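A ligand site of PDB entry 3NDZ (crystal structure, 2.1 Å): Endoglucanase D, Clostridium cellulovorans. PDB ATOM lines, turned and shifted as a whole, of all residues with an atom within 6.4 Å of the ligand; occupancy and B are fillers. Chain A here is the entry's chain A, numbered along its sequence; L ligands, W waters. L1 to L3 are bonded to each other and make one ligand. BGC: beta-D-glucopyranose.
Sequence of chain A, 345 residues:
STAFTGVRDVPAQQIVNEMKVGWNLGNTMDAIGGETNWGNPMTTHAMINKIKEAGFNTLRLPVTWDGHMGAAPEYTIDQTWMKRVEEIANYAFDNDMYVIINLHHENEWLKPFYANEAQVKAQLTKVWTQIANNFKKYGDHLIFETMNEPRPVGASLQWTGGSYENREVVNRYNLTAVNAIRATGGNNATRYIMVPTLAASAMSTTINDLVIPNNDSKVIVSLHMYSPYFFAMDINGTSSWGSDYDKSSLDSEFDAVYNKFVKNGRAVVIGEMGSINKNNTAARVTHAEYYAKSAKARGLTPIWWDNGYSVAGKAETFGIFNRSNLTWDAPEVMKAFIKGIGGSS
Water W2 lies within hydrogen-bond range of OD2 of Asp 30 (2.7 Å), NE2 of His 105 (2.8 Å), O3 of BGC L1 (2.8 Å) and OD1 of Asn 27 (2.9 Å). Water W3 bridges OE2 of Glu 149 and O1 of BGC L1.
ND2 of Asn 307 lies within hydrogen-bond range of O of Glu 316 (2.8 Å). The side-chain amide nitrogen (ND2) of Asn 148 sits close to the guanidinium group (NH2) of Arg 60, 2.9 Å away. NH2 of Arg 151 lies within salt-bridge range of OE1 of Glu 149, at 3.2 Å. The backbone carbonyl oxygen of Tyr 309 is in hydrogen-bond range of the backbone NH of Phe 318 (3.3 Å). The side-chain amide nitrogen (ND2) of Asn 148 lies close to a ring nitrogen (ND1) of His 104. The side-chain carboxylate of Glu 272 is in salt-bridge range of the guanidinium group of Arg 60, 2.8 Å away. The side-chain amide oxygen (OD1) of Asn 307 is in hydrogen-bond range of the backbone NH (N) of Tyr 309. OE1 of Glu 272 lies close to ND1 of His 224 (3.4 Å).
Trp 38 touches the ligand. OH of Tyr 226 touches C5 of BGC L1 (3.6 Å). CE of Met 233 touches C6 of BGC L1 (3.98 Å). Phe 318 touches the ligand. Hydrophobic or aromatic side chains within 4 Å of the ligand: Trp 38, His 104, His 105, Met 233, Trp 305 and Phe 318. Within 4 Å of the ligand: Asn 27, Trp 38, His 104, His 105, Asn 148, Glu 149, Tyr 226, Met 233, Glu 272, Trp 305, Asn 307, Glu 316 and Phe 318. The nearest printed residue that does not touch the ligand is His 224 (4.3 Å).
OE2 of Glu 272 is in hydrogen-bond range of O2 of BGC L1, 3.1 Å away. An oxygen (O2) of BGC L1 lies within hydrogen-bond range of the side-chain amide oxygen (OD1) of Asn 148, 3.1 Å away. The side-chain carboxylate (OE1) of Glu 316 sits at hydrogen-bond distance from an oxygen (O2) of BGC L2 (3.0 Å). An oxygen (O1) of BGC L1 sits at hydrogen-bond distance from the side-chain carboxylate (OE2) of Glu 149 (2.5 Å). O2 of BGC L2 is in hydrogen-bond range of ND2 of Asn 307 (2.8 Å). ND2 of Asn 27 sits at hydrogen-bond distance from O3 of BGC L2, at 2.9 Å. NE2 of His 104 sits at hydrogen-bond distance from O3 of BGC L1 (2.9 Å). A ring nitrogen (NE2) of His 105 sits close to an oxygen (O3) of BGC L1 (3.4 Å). The indole nitrogen (NE1) of Trp 305 sits at hydrogen-bond distance from an oxygen (O2) of BGC L2, at 3.1 Å.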
ATOM      1  N   ASN A  27       1.085   1.478  10.074  1.00  0.00           N
ATOM      2  CA  ASN A  27       0.161   1.750  11.172  1.00  0.00           C
ATOM      3  C   ASN A  27       0.119   0.611  12.148  1.00  0.00           C
ATOM      4  O   ASN A  27      -0.946   0.250  12.659  1.00  0.00           O
ATOM      5  CB  ASN A  27      -1.256   2.066  10.649  1.00  0.00           C
ATOM      6  CG  ASN A  27      -1.404   3.513  10.245  1.00  0.00           C
ATOM      7  OD1 ASN A  27      -0.409   4.230  10.077  1.00  0.00           O
ATOM      8  ND2 ASN A  27      -2.643   3.963  10.095  1.00  0.00           N
ATOM      9  N   ASP A  30       4.701   1.129  14.043  1.00  0.00           N
ATOM     10  CA  ASP A  30       4.856   2.581  13.942  1.00  0.00           C
ATOM     11  C   ASP A  30       3.715   3.365  14.611  1.00  0.00           C
ATOM     12  O   ASP A  30       3.814   4.578  14.782  1.00  0.00           O
ATOM     13  CB  ASP A  30       4.968   2.994  12.462  1.00  0.00           C
ATOM     14  CG  ASP A  30       3.845   2.402  11.599  1.00  0.00           C
ATOM     15  OD1 ASP A  30       3.599   1.178  11.684  1.00  0.00           O
ATOM     16  OD2 ASP A  30       3.227   3.164  10.817  1.00  0.00           O
ATOM     17  N   ASN A  37      -2.891  -0.068  18.367  1.00  0.00           N
ATOM     18  CA  ASN A  37      -3.534   1.169  18.755  1.00  0.00           C
ATOM     19  C   ASN A  37      -4.174   1.952  17.619  1.00  0.00           C
ATOM     20  O   ASN A  37      -4.997   2.830  17.860  1.00  0.00           O
ATOM     21  CB  ASN A  37      -2.552   2.070  19.487  1.00  0.00           C
ATOM     22  CG  ASN A  37      -3.251   3.169  20.245  1.00  0.00           C
ATOM     23  OD1 ASN A  37      -4.289   2.938  20.861  1.00  0.00           O
ATOM     24  ND2 ASN A  37      -2.711   4.375  20.197  1.00  0.00           N
ATOM     25  N   TRP A  38      -3.795   1.643  16.385  1.00  0.00           N
ATOM     26  CA  TRP A  38      -4.350   2.347  15.238  1.00  0.00           C
ATOM     27  C   TRP A  38      -5.221   1.447  14.369  1.00  0.00           C
ATOM     28  O   TRP A  38      -5.338   1.644  13.161  1.00  0.00           O
ATOM     29  CB  TRP A  38      -3.244   3.013  14.407  1.00  0.00           C
ATOM     30  CG  TRP A  38      -2.718   4.287  15.033  1.00  0.00           C
ATOM     31  CD1 TRP A  38      -3.147   4.883  16.182  1.00  0.00           C
ATOM     32  CD2 TRP A  38      -1.657   5.119  14.522  1.00  0.00           C
ATOM     33  NE1 TRP A  38      -2.428   6.027  16.431  1.00  0.00           N
ATOM     34  CE2 TRP A  38      -1.503   6.199  15.432  1.00  0.00           C
ATOM     35  CE3 TRP A  38      -0.826   5.058  13.397  1.00  0.00           C
ATOM     36  CZ2 TRP A  38      -0.547   7.208  15.238  1.00  0.00           C
ATOM     37  CZ3 TRP A  38       0.117   6.064  13.209  1.00  0.00           C
ATOM     38  CH2 TRP A  38       0.241   7.125  14.133  1.00  0.00           C
ATOM     39  N   GLY A  39      -5.844   0.451  15.000  1.00  0.00           N
ATOM     40  CA  GLY A  39      -6.840  -0.350  14.320  1.00  0.00           C
ATOM     41  C   GLY A  39      -6.394  -1.575  13.541  1.00  0.00           C
ATOM     42  O   GLY A  39      -7.210  -2.240  12.900  1.00  0.00           O
ATOM     43  N   ARG A  60       8.996  -4.053   4.740  1.00  0.00           N
ATOM     44  CA  ARG A  60       9.443  -2.915   5.523  1.00  0.00           C
ATOM     45  C   ARG A  60       8.637  -2.895   6.795  1.00  0.00           C
ATOM     46  O   ARG A  60       7.410  -2.991   6.775  1.00  0.00           O
ATOM     47  CB  ARG A  60       9.328  -1.580   4.781  1.00  0.00           C
ATOM     48  CG  ARG A  60       9.833  -0.357   5.609  1.00  0.00           C
ATOM     49  CD  ARG A  60       9.985   0.856   4.665  1.00  0.00           C
ATOM     50  NE  ARG A  60      10.459   2.111   5.258  1.00  0.00           N
ATOM     51  CZ  ARG A  60       9.670   3.094   5.704  1.00  0.00           C
ATOM     52  NH1 ARG A  60       8.348   2.951   5.664  1.00  0.00           N
ATOM     53  NH2 ARG A  60      10.195   4.222   6.174  1.00  0.00           N
ATOM     54  N   HIS A 104      10.579   5.508  13.195  1.00  0.00           N
ATOM     55  CA  HIS A 104       9.490   6.092  12.398  1.00  0.00           C
ATOM     56  C   HIS A 104       8.965   7.439  12.885  1.00  0.00           C
ATOM     57  O   HIS A 104       9.524   8.484  12.549  1.00  0.00           O
ATOM     58  CB  HIS A 104       8.362   5.081  12.214  1.00  0.00           C
ATOM     59  CG  HIS A 104       7.584   5.287  10.946  1.00  0.00           C
ATOM     60  ND1 HIS A 104       8.106   4.992   9.701  1.00  0.00           N
ATOM     61  CD2 HIS A 104       6.337   5.776  10.730  1.00  0.00           C
ATOM     62  CE1 HIS A 104       7.210   5.278   8.780  1.00  0.00           C
ATOM     63  NE2 HIS A 104       6.125   5.759   9.370  1.00  0.00           N
ATOM     64  N   HIS A 105       7.887   7.434  13.660  1.00  0.00           N
ATOM     65  CA  HIS A 105       7.279   8.672  14.139  1.00  0.00           C
ATOM     66  C   HIS A 105       7.977   9.247  15.379  1.00  0.00           C
ATOM     67  O   HIS A 105       7.393   9.323  16.456  1.00  0.00           O
ATOM     68  CB  HIS A 105       5.792   8.473  14.446  1.00  0.00           C
ATOM     69  CG  HIS A 105       4.936   8.255  13.232  1.00  0.00           C
ATOM     70  ND1 HIS A 105       5.022   9.041  12.112  1.00  0.00           N
ATOM     71  CD2 HIS A 105       3.975   7.332  12.970  1.00  0.00           C
ATOM     72  CE1 HIS A 105       4.148   8.629  11.203  1.00  0.00           C
ATOM     73  NE2 HIS A 105       3.505   7.585  11.702  1.00  0.00           N
ATOM     74  N   ASN A 148      13.108   8.026   9.405  1.00  0.00           N
ATOM     75  CA  ASN A 148      11.998   7.958   8.470  1.00  0.00           C
ATOM     76  C   ASN A 148      11.916   9.224   7.614  1.00  0.00           C
ATOM     77  O   ASN A 148      12.414   9.258   6.492  1.00  0.00           O
ATOM     78  CB  ASN A 148      10.690   7.771   9.243  1.00  0.00           C
ATOM     79  CG  ASN A 148       9.489   7.614   8.324  1.00  0.00           C
ATOM     80  OD1 ASN A 148       8.424   8.202   8.573  1.00  0.00           O
ATOM     81  ND2 ASN A 148       9.633   6.819   7.270  1.00  0.00           N
ATOM     82  N   GLU A 149      11.305  10.269   8.162  1.00  0.00           N
ATOM     83  CA  GLU A 149      11.163  11.526   7.444  1.00  0.00           C
ATOM     84  C   GLU A 149      11.537  12.729   8.321  1.00  0.00           C
ATOM     85  O   GLU A 149      10.697  13.582   8.615  1.00  0.00           O
ATOM     86  CB  GLU A 149       9.747  11.683   6.897  1.00  0.00           C
ATOM     87  CG  GLU A 149       9.448  10.714   5.752  1.00  0.00           C
ATOM     88  CD  GLU A 149       8.101  10.962   5.091  1.00  0.00           C
ATOM     89  OE1 GLU A 149       7.414  11.948   5.450  1.00  0.00           O
ATOM     90  OE2 GLU A 149       7.729  10.166   4.196  1.00  0.00           O
ATOM     91  N   ARG A 151      12.448  16.178   9.598  1.00  0.00           N
ATOM     92  CA  ARG A 151      12.032  17.426   8.973  1.00  0.00           C
ATOM     93  C   ARG A 151      11.636  18.428  10.050  1.00  0.00           C
ATOM     94  O   ARG A 151      11.333  18.036  11.174  1.00  0.00           O
ATOM     95  CB  ARG A 151      10.806  17.142   8.108  1.00  0.00           C
ATOM     96  CG  ARG A 151       9.665  16.585   8.953  1.00  0.00           C
ATOM     97  CD  ARG A 151       8.287  16.852   8.372  1.00  0.00           C
ATOM     98  NE  ARG A 151       7.889  15.858   7.375  1.00  0.00           N
ATOM     99  CZ  ARG A 151       7.703  16.133   6.093  1.00  0.00           C
ATOM    100  NH1 ARG A 151       7.887  17.385   5.654  1.00  0.00           N
ATOM    101  NH2 ARG A 151       7.323  15.190   5.243  1.00  0.00           N
ATOM    102  N   ALA A 199      12.952  14.741   5.025  1.00  0.00           N
ATOM    103  CA  ALA A 199      11.593  14.303   4.746  1.00  0.00           C
ATOM    104  C   ALA A 199      11.527  13.093   3.790  1.00  0.00           C
ATOM    105  O   ALA A 199      10.468  12.772   3.274  1.00  0.00           O
ATOM    106  CB  ALA A 199      10.741  15.459   4.220  1.00  0.00           C
ATOM    107  N   HIS A 224      10.733   8.547  -0.238  1.00  0.00           N
ATOM    108  CA  HIS A 224       9.311   8.250  -0.259  1.00  0.00           C
ATOM    109  C   HIS A 224       8.702   9.031  -1.398  1.00  0.00           C
ATOM    110  O   HIS A 224       8.822  10.256  -1.429  1.00  0.00           O
ATOM    111  CB  HIS A 224       8.679   8.597   1.084  1.00  0.00           C
ATOM    112  CG  HIS A 224       9.216   7.787   2.224  1.00  0.00           C
ATOM    113  ND1 HIS A 224       8.864   7.986   3.545  1.00  0.00           N
ATOM    114  CD2 HIS A 224      10.082   6.740   2.227  1.00  0.00           C
ATOM    115  CE1 HIS A 224       9.488   7.116   4.302  1.00  0.00           C
ATOM    116  NE2 HIS A 224      10.241   6.348   3.533  1.00  0.00           N
ATOM    117  N   TYR A 226       5.186   9.239  -3.156  1.00  0.00           N
ATOM    118  CA  TYR A 226       3.768   9.034  -3.446  1.00  0.00           C
ATOM    119  C   TYR A 226       3.349   9.881  -4.655  1.00  0.00           C
ATOM    120  O   TYR A 226       2.658  10.874  -4.487  1.00  0.00           O
ATOM    121  CB  TYR A 226       2.922   9.429  -2.242  1.00  0.00           C
ATOM    122  CG  TYR A 226       3.106   8.598  -0.997  1.00  0.00           C
ATOM    123  CD1 TYR A 226       2.244   7.527  -0.720  1.00  0.00           C
ATOM    124  CD2 TYR A 226       4.093   8.896  -0.074  1.00  0.00           C
ATOM    125  CE1 TYR A 226       2.392   6.770   0.435  1.00  0.00           C
ATOM    126  CE2 TYR A 226       4.250   8.137   1.083  1.00  0.00           C
ATOM    127  CZ  TYR A 226       3.397   7.082   1.336  1.00  0.00           C
ATOM    128  OH  TYR A 226       3.546   6.333   2.498  1.00  0.00           O
ATOM    129  N   MET A 233      -2.448  10.699  -3.335  1.00  0.00           N
ATOM    130  CA  MET A 233      -2.558  11.066  -1.929  1.00  0.00           C
ATOM    131  C   MET A 233      -3.754  11.940  -1.565  1.00  0.00           C
ATOM    132  O   MET A 233      -4.263  11.865  -0.438  1.00  0.00           O
ATOM    133  CB  MET A 233      -1.271  11.789  -1.513  1.00  0.00           C
ATOM    134  CG  MET A 233      -0.859  11.551  -0.089  1.00  0.00           C
ATOM    135  SD  MET A 233       0.924  11.819  -0.012  1.00  0.00           S
ATOM    136  CE  MET A 233       1.381  10.543   1.138  1.00  0.00           C
ATOM    137  N   GLU A 272       8.423   3.978   0.569  1.00  0.00           N
ATOM    138  CA  GLU A 272       6.984   4.176   0.650  1.00  0.00           C
ATOM    139  C   GLU A 272       6.468   4.776  -0.633  1.00  0.00           C
ATOM    140  O   GLU A 272       7.056   5.703  -1.184  1.00  0.00           O
ATOM    141  CB  GLU A 272       6.611   5.101   1.824  1.00  0.00           C
ATOM    142  CG  GLU A 272       7.007   4.586   3.198  1.00  0.00           C
ATOM    143  CD  GLU A 272       6.568   5.539   4.314  1.00  0.00           C
ATOM    144  OE1 GLU A 272       5.803   6.481   4.017  1.00  0.00           O
ATOM    145  OE2 GLU A 272       6.970   5.345   5.469  1.00  0.00           O
ATOM    146  N   TRP A 305       2.988   1.354   0.640  1.00  0.00           N
ATOM    147  CA  TRP A 305       2.562   1.721   1.987  1.00  0.00           C
ATOM    148  C   TRP A 305       1.195   1.110   2.266  1.00  0.00           C
ATOM    149  O   TRP A 305       0.207   1.490   1.634  1.00  0.00           O
ATOM    150  CB  TRP A 305       2.504   3.244   2.163  1.00  0.00           C
ATOM    151  CG  TRP A 305       2.054   3.658   3.535  1.00  0.00           C
ATOM    152  CD1 TRP A 305       0.874   4.263   3.867  1.00  0.00           C
ATOM    153  CD2 TRP A 305       2.773   3.482   4.775  1.00  0.00           C
ATOM    154  NE1 TRP A 305       0.812   4.476   5.234  1.00  0.00           N
ATOM    155  CE2 TRP A 305       1.963   4.002   5.811  1.00  0.00           C
ATOM    156  CE3 TRP A 305       4.019   2.918   5.105  1.00  0.00           C
ATOM    157  CZ2 TRP A 305       2.367   3.980   7.153  1.00  0.00           C
ATOM    158  CZ3 TRP A 305       4.425   2.904   6.454  1.00  0.00           C
ATOM    159  CH2 TRP A 305       3.594   3.441   7.455  1.00  0.00           C
ATOM    160  N   ASN A 307      -1.419   0.624   5.243  1.00  0.00           N
ATOM    161  CA  ASN A 307      -1.733   0.970   6.632  1.00  0.00           C
ATOM    162  C   ASN A 307      -2.952   0.197   7.176  1.00  0.00           C
ATOM    163  O   ASN A 307      -3.418   0.458   8.290  1.00  0.00           O
ATOM    164  CB  ASN A 307      -1.918   2.476   6.785  1.00  0.00           C
ATOM    165  CG  ASN A 307      -3.094   3.003   5.979  1.00  0.00           C
ATOM    166  OD1 ASN A 307      -3.722   2.259   5.226  1.00  0.00           O
ATOM    167  ND2 ASN A 307      -3.407   4.289   6.144  1.00  0.00           N
ATOM    168  N   TYR A 309      -5.987   0.165   5.976  1.00  0.00           N
ATOM    169  CA  TYR A 309      -7.232   0.911   5.854  1.00  0.00           C
ATOM    170  C   TYR A 309      -7.555   1.054   4.372  1.00  0.00           C
ATOM    171  O   TYR A 309      -6.811   1.703   3.643  1.00  0.00           O
ATOM    172  CB  TYR A 309      -7.077   2.280   6.520  1.00  0.00           C
ATOM    173  CG  TYR A 309      -8.359   3.080   6.616  1.00  0.00           C
ATOM    174  CD1 TYR A 309      -9.550   2.478   6.983  1.00  0.00           C
ATOM    175  CD2 TYR A 309      -8.366   4.449   6.354  1.00  0.00           C
ATOM    176  CE1 TYR A 309     -10.731   3.216   7.074  1.00  0.00           C
ATOM    177  CE2 TYR A 309      -9.547   5.196   6.451  1.00  0.00           C
ATOM    178  CZ  TYR A 309     -10.711   4.570   6.812  1.00  0.00           C
ATOM    179  OH  TYR A 309     -11.888   5.293   6.906  1.00  0.00           O
ATOM    180  N   GLU A 316      -6.309   8.683   3.156  1.00  0.00           N
ATOM    181  CA  GLU A 316      -5.342   7.762   3.754  1.00  0.00           C
ATOM    182  C   GLU A 316      -5.695   6.294   3.597  1.00  0.00           C
ATOM    183  O   GLU A 316      -5.264   5.472   4.391  1.00  0.00           O
ATOM    184  CB  GLU A 316      -5.163   8.088   5.244  1.00  0.00           C
ATOM    185  CG  GLU A 316      -4.647   9.490   5.508  1.00  0.00           C
ATOM    186  CD  GLU A 316      -3.217   9.679   5.041  1.00  0.00           C
ATOM    187  OE1 GLU A 316      -2.423   8.713   5.100  1.00  0.00           O
ATOM    188  OE2 GLU A 316      -2.870  10.808   4.617  1.00  0.00           O
ATOM    189  N   PHE A 318      -4.665   3.678   2.013  1.00  0.00           N
ATOM    190  CA  PHE A 318      -3.578   3.057   1.259  1.00  0.00           C
ATOM    191  C   PHE A 318      -3.565   1.533   1.374  1.00  0.00           C
ATOM    192  O   PHE A 318      -2.780   0.873   0.706  1.00  0.00           O
ATOM    193  CB  PHE A 318      -2.225   3.575   1.747  1.00  0.00           C
ATOM    194  CG  PHE A 318      -1.938   4.993   1.403  1.00  0.00           C
ATOM    195  CD1 PHE A 318      -2.039   5.994   2.364  1.00  0.00           C
ATOM    196  CD2 PHE A 318      -1.542   5.352   0.124  1.00  0.00           C
ATOM    197  CE1 PHE A 318      -1.751   7.318   2.043  1.00  0.00           C
ATOM    198  CE2 PHE A 318      -1.256   6.668  -0.203  1.00  0.00           C
ATOM    199  CZ  PHE A 318      -1.362   7.657   0.773  1.00  0.00           C
HETATM  200  C2  BGC L   1       4.624   8.501   6.665  1.00  0.00           C
HETATM  201  C3  BGC L   1       3.612   7.414   6.988  1.00  0.00           C
HETATM  202  C4  BGC L   1       2.238   8.008   6.707  1.00  0.00           C
HETATM  203  C5  BGC L   1       2.096   8.370   5.155  1.00  0.00           C
HETATM  204  C6  BGC L   1       0.721   8.931   4.720  1.00  0.00           C
HETATM  205  C1  BGC L   1       4.442   8.858   5.210  1.00  0.00           C
HETATM  206  O1  BGC L   1       5.319   9.966   4.966  1.00  0.00           O
HETATM  207  O2  BGC L   1       5.924   7.918   6.796  1.00  0.00           O
HETATM  208  O3  BGC L   1       3.713   7.058   8.373  1.00  0.00           O
HETATM  209  O4  BGC L   1       1.276   7.015   7.013  1.00  0.00           O
HETATM  210  O5  BGC L   1       3.128   9.358   4.860  1.00  0.00           O
HETATM  211  O6  BGC L   1       0.375  10.133   5.380  1.00  0.00           O
HETATM  212  C2  BGC L   2      -0.972   6.648   7.792  1.00  0.00           C
HETATM  213  C3  BGC L   2      -2.106   7.394   8.475  1.00  0.00           C
HETATM  214  C4  BGC L   2      -1.617   7.879   9.853  1.00  0.00           C
HETATM  215  C5  BGC L   2      -0.454   8.811   9.672  1.00  0.00           C
HETATM  216  C6  BGC L   2       0.017   9.151  11.093  1.00  0.00           C
HETATM  217  C1  BGC L   2       0.176   7.664   7.653  1.00  0.00           C
HETATM  218  O2  BGC L   2      -1.375   6.212   6.483  1.00  0.00           O
HETATM  219  O3  BGC L   2      -3.182   6.473   8.659  1.00  0.00           O
HETATM  220  O4  BGC L   2      -2.600   8.611  10.611  1.00  0.00           O
HETATM  221  O5  BGC L   2       0.605   8.131   8.981  1.00  0.00           O
HETATM  222  O6  BGC L   2       1.114  10.082  11.041  1.00  0.00           O
HETATM  223  C2  BGC L   3      -3.710   9.305  12.595  1.00  0.00           C
HETATM  224  C3  BGC L   3      -4.145   8.845  13.980  1.00  0.00           C
HETATM  225  C4  BGC L   3      -5.131   7.720  13.769  1.00  0.00           C
HETATM  226  C5  BGC L   3      -4.442   6.578  13.003  1.00  0.00           C
HETATM  227  C6  BGC L   3      -5.441   5.462  12.652  1.00  0.00           C
HETATM  228  C1  BGC L   3      -3.018   8.140  11.891  1.00  0.00           C
HETATM  229  O2  BGC L   3      -2.767  10.373  12.722  1.00  0.00           O
HETATM  230  O3  BGC L   3      -4.772   9.908  14.688  1.00  0.00           O
HETATM  231  O4  BGC L   3      -5.567   7.263  15.052  1.00  0.00           O
HETATM  232  O5  BGC L   3      -3.975   7.071  11.719  1.00  0.00           O
HETATM  233  O6  BGC L   3      -6.461   5.996  11.808  1.00  0.00           O
HETATM  234  O   HOH W   1      -5.607   7.407   9.410  1.00  0.00           O
HETATM  235  O   HOH W   2       2.179   5.600  10.278  1.00  0.00           O
HETATM  236  O   HOH W   3       5.578  11.355   1.828  1.00  0.00           O
HETATM  237  O   HOH W   4       2.181  10.771  13.849  1.00  0.00           O
HETATM  238  O   HOH W   5      -2.468  12.219  10.779  1.00  0.00           O
HETATM  239  O   HOH W   6      -0.418  11.032  14.631  1.00  0.00           O
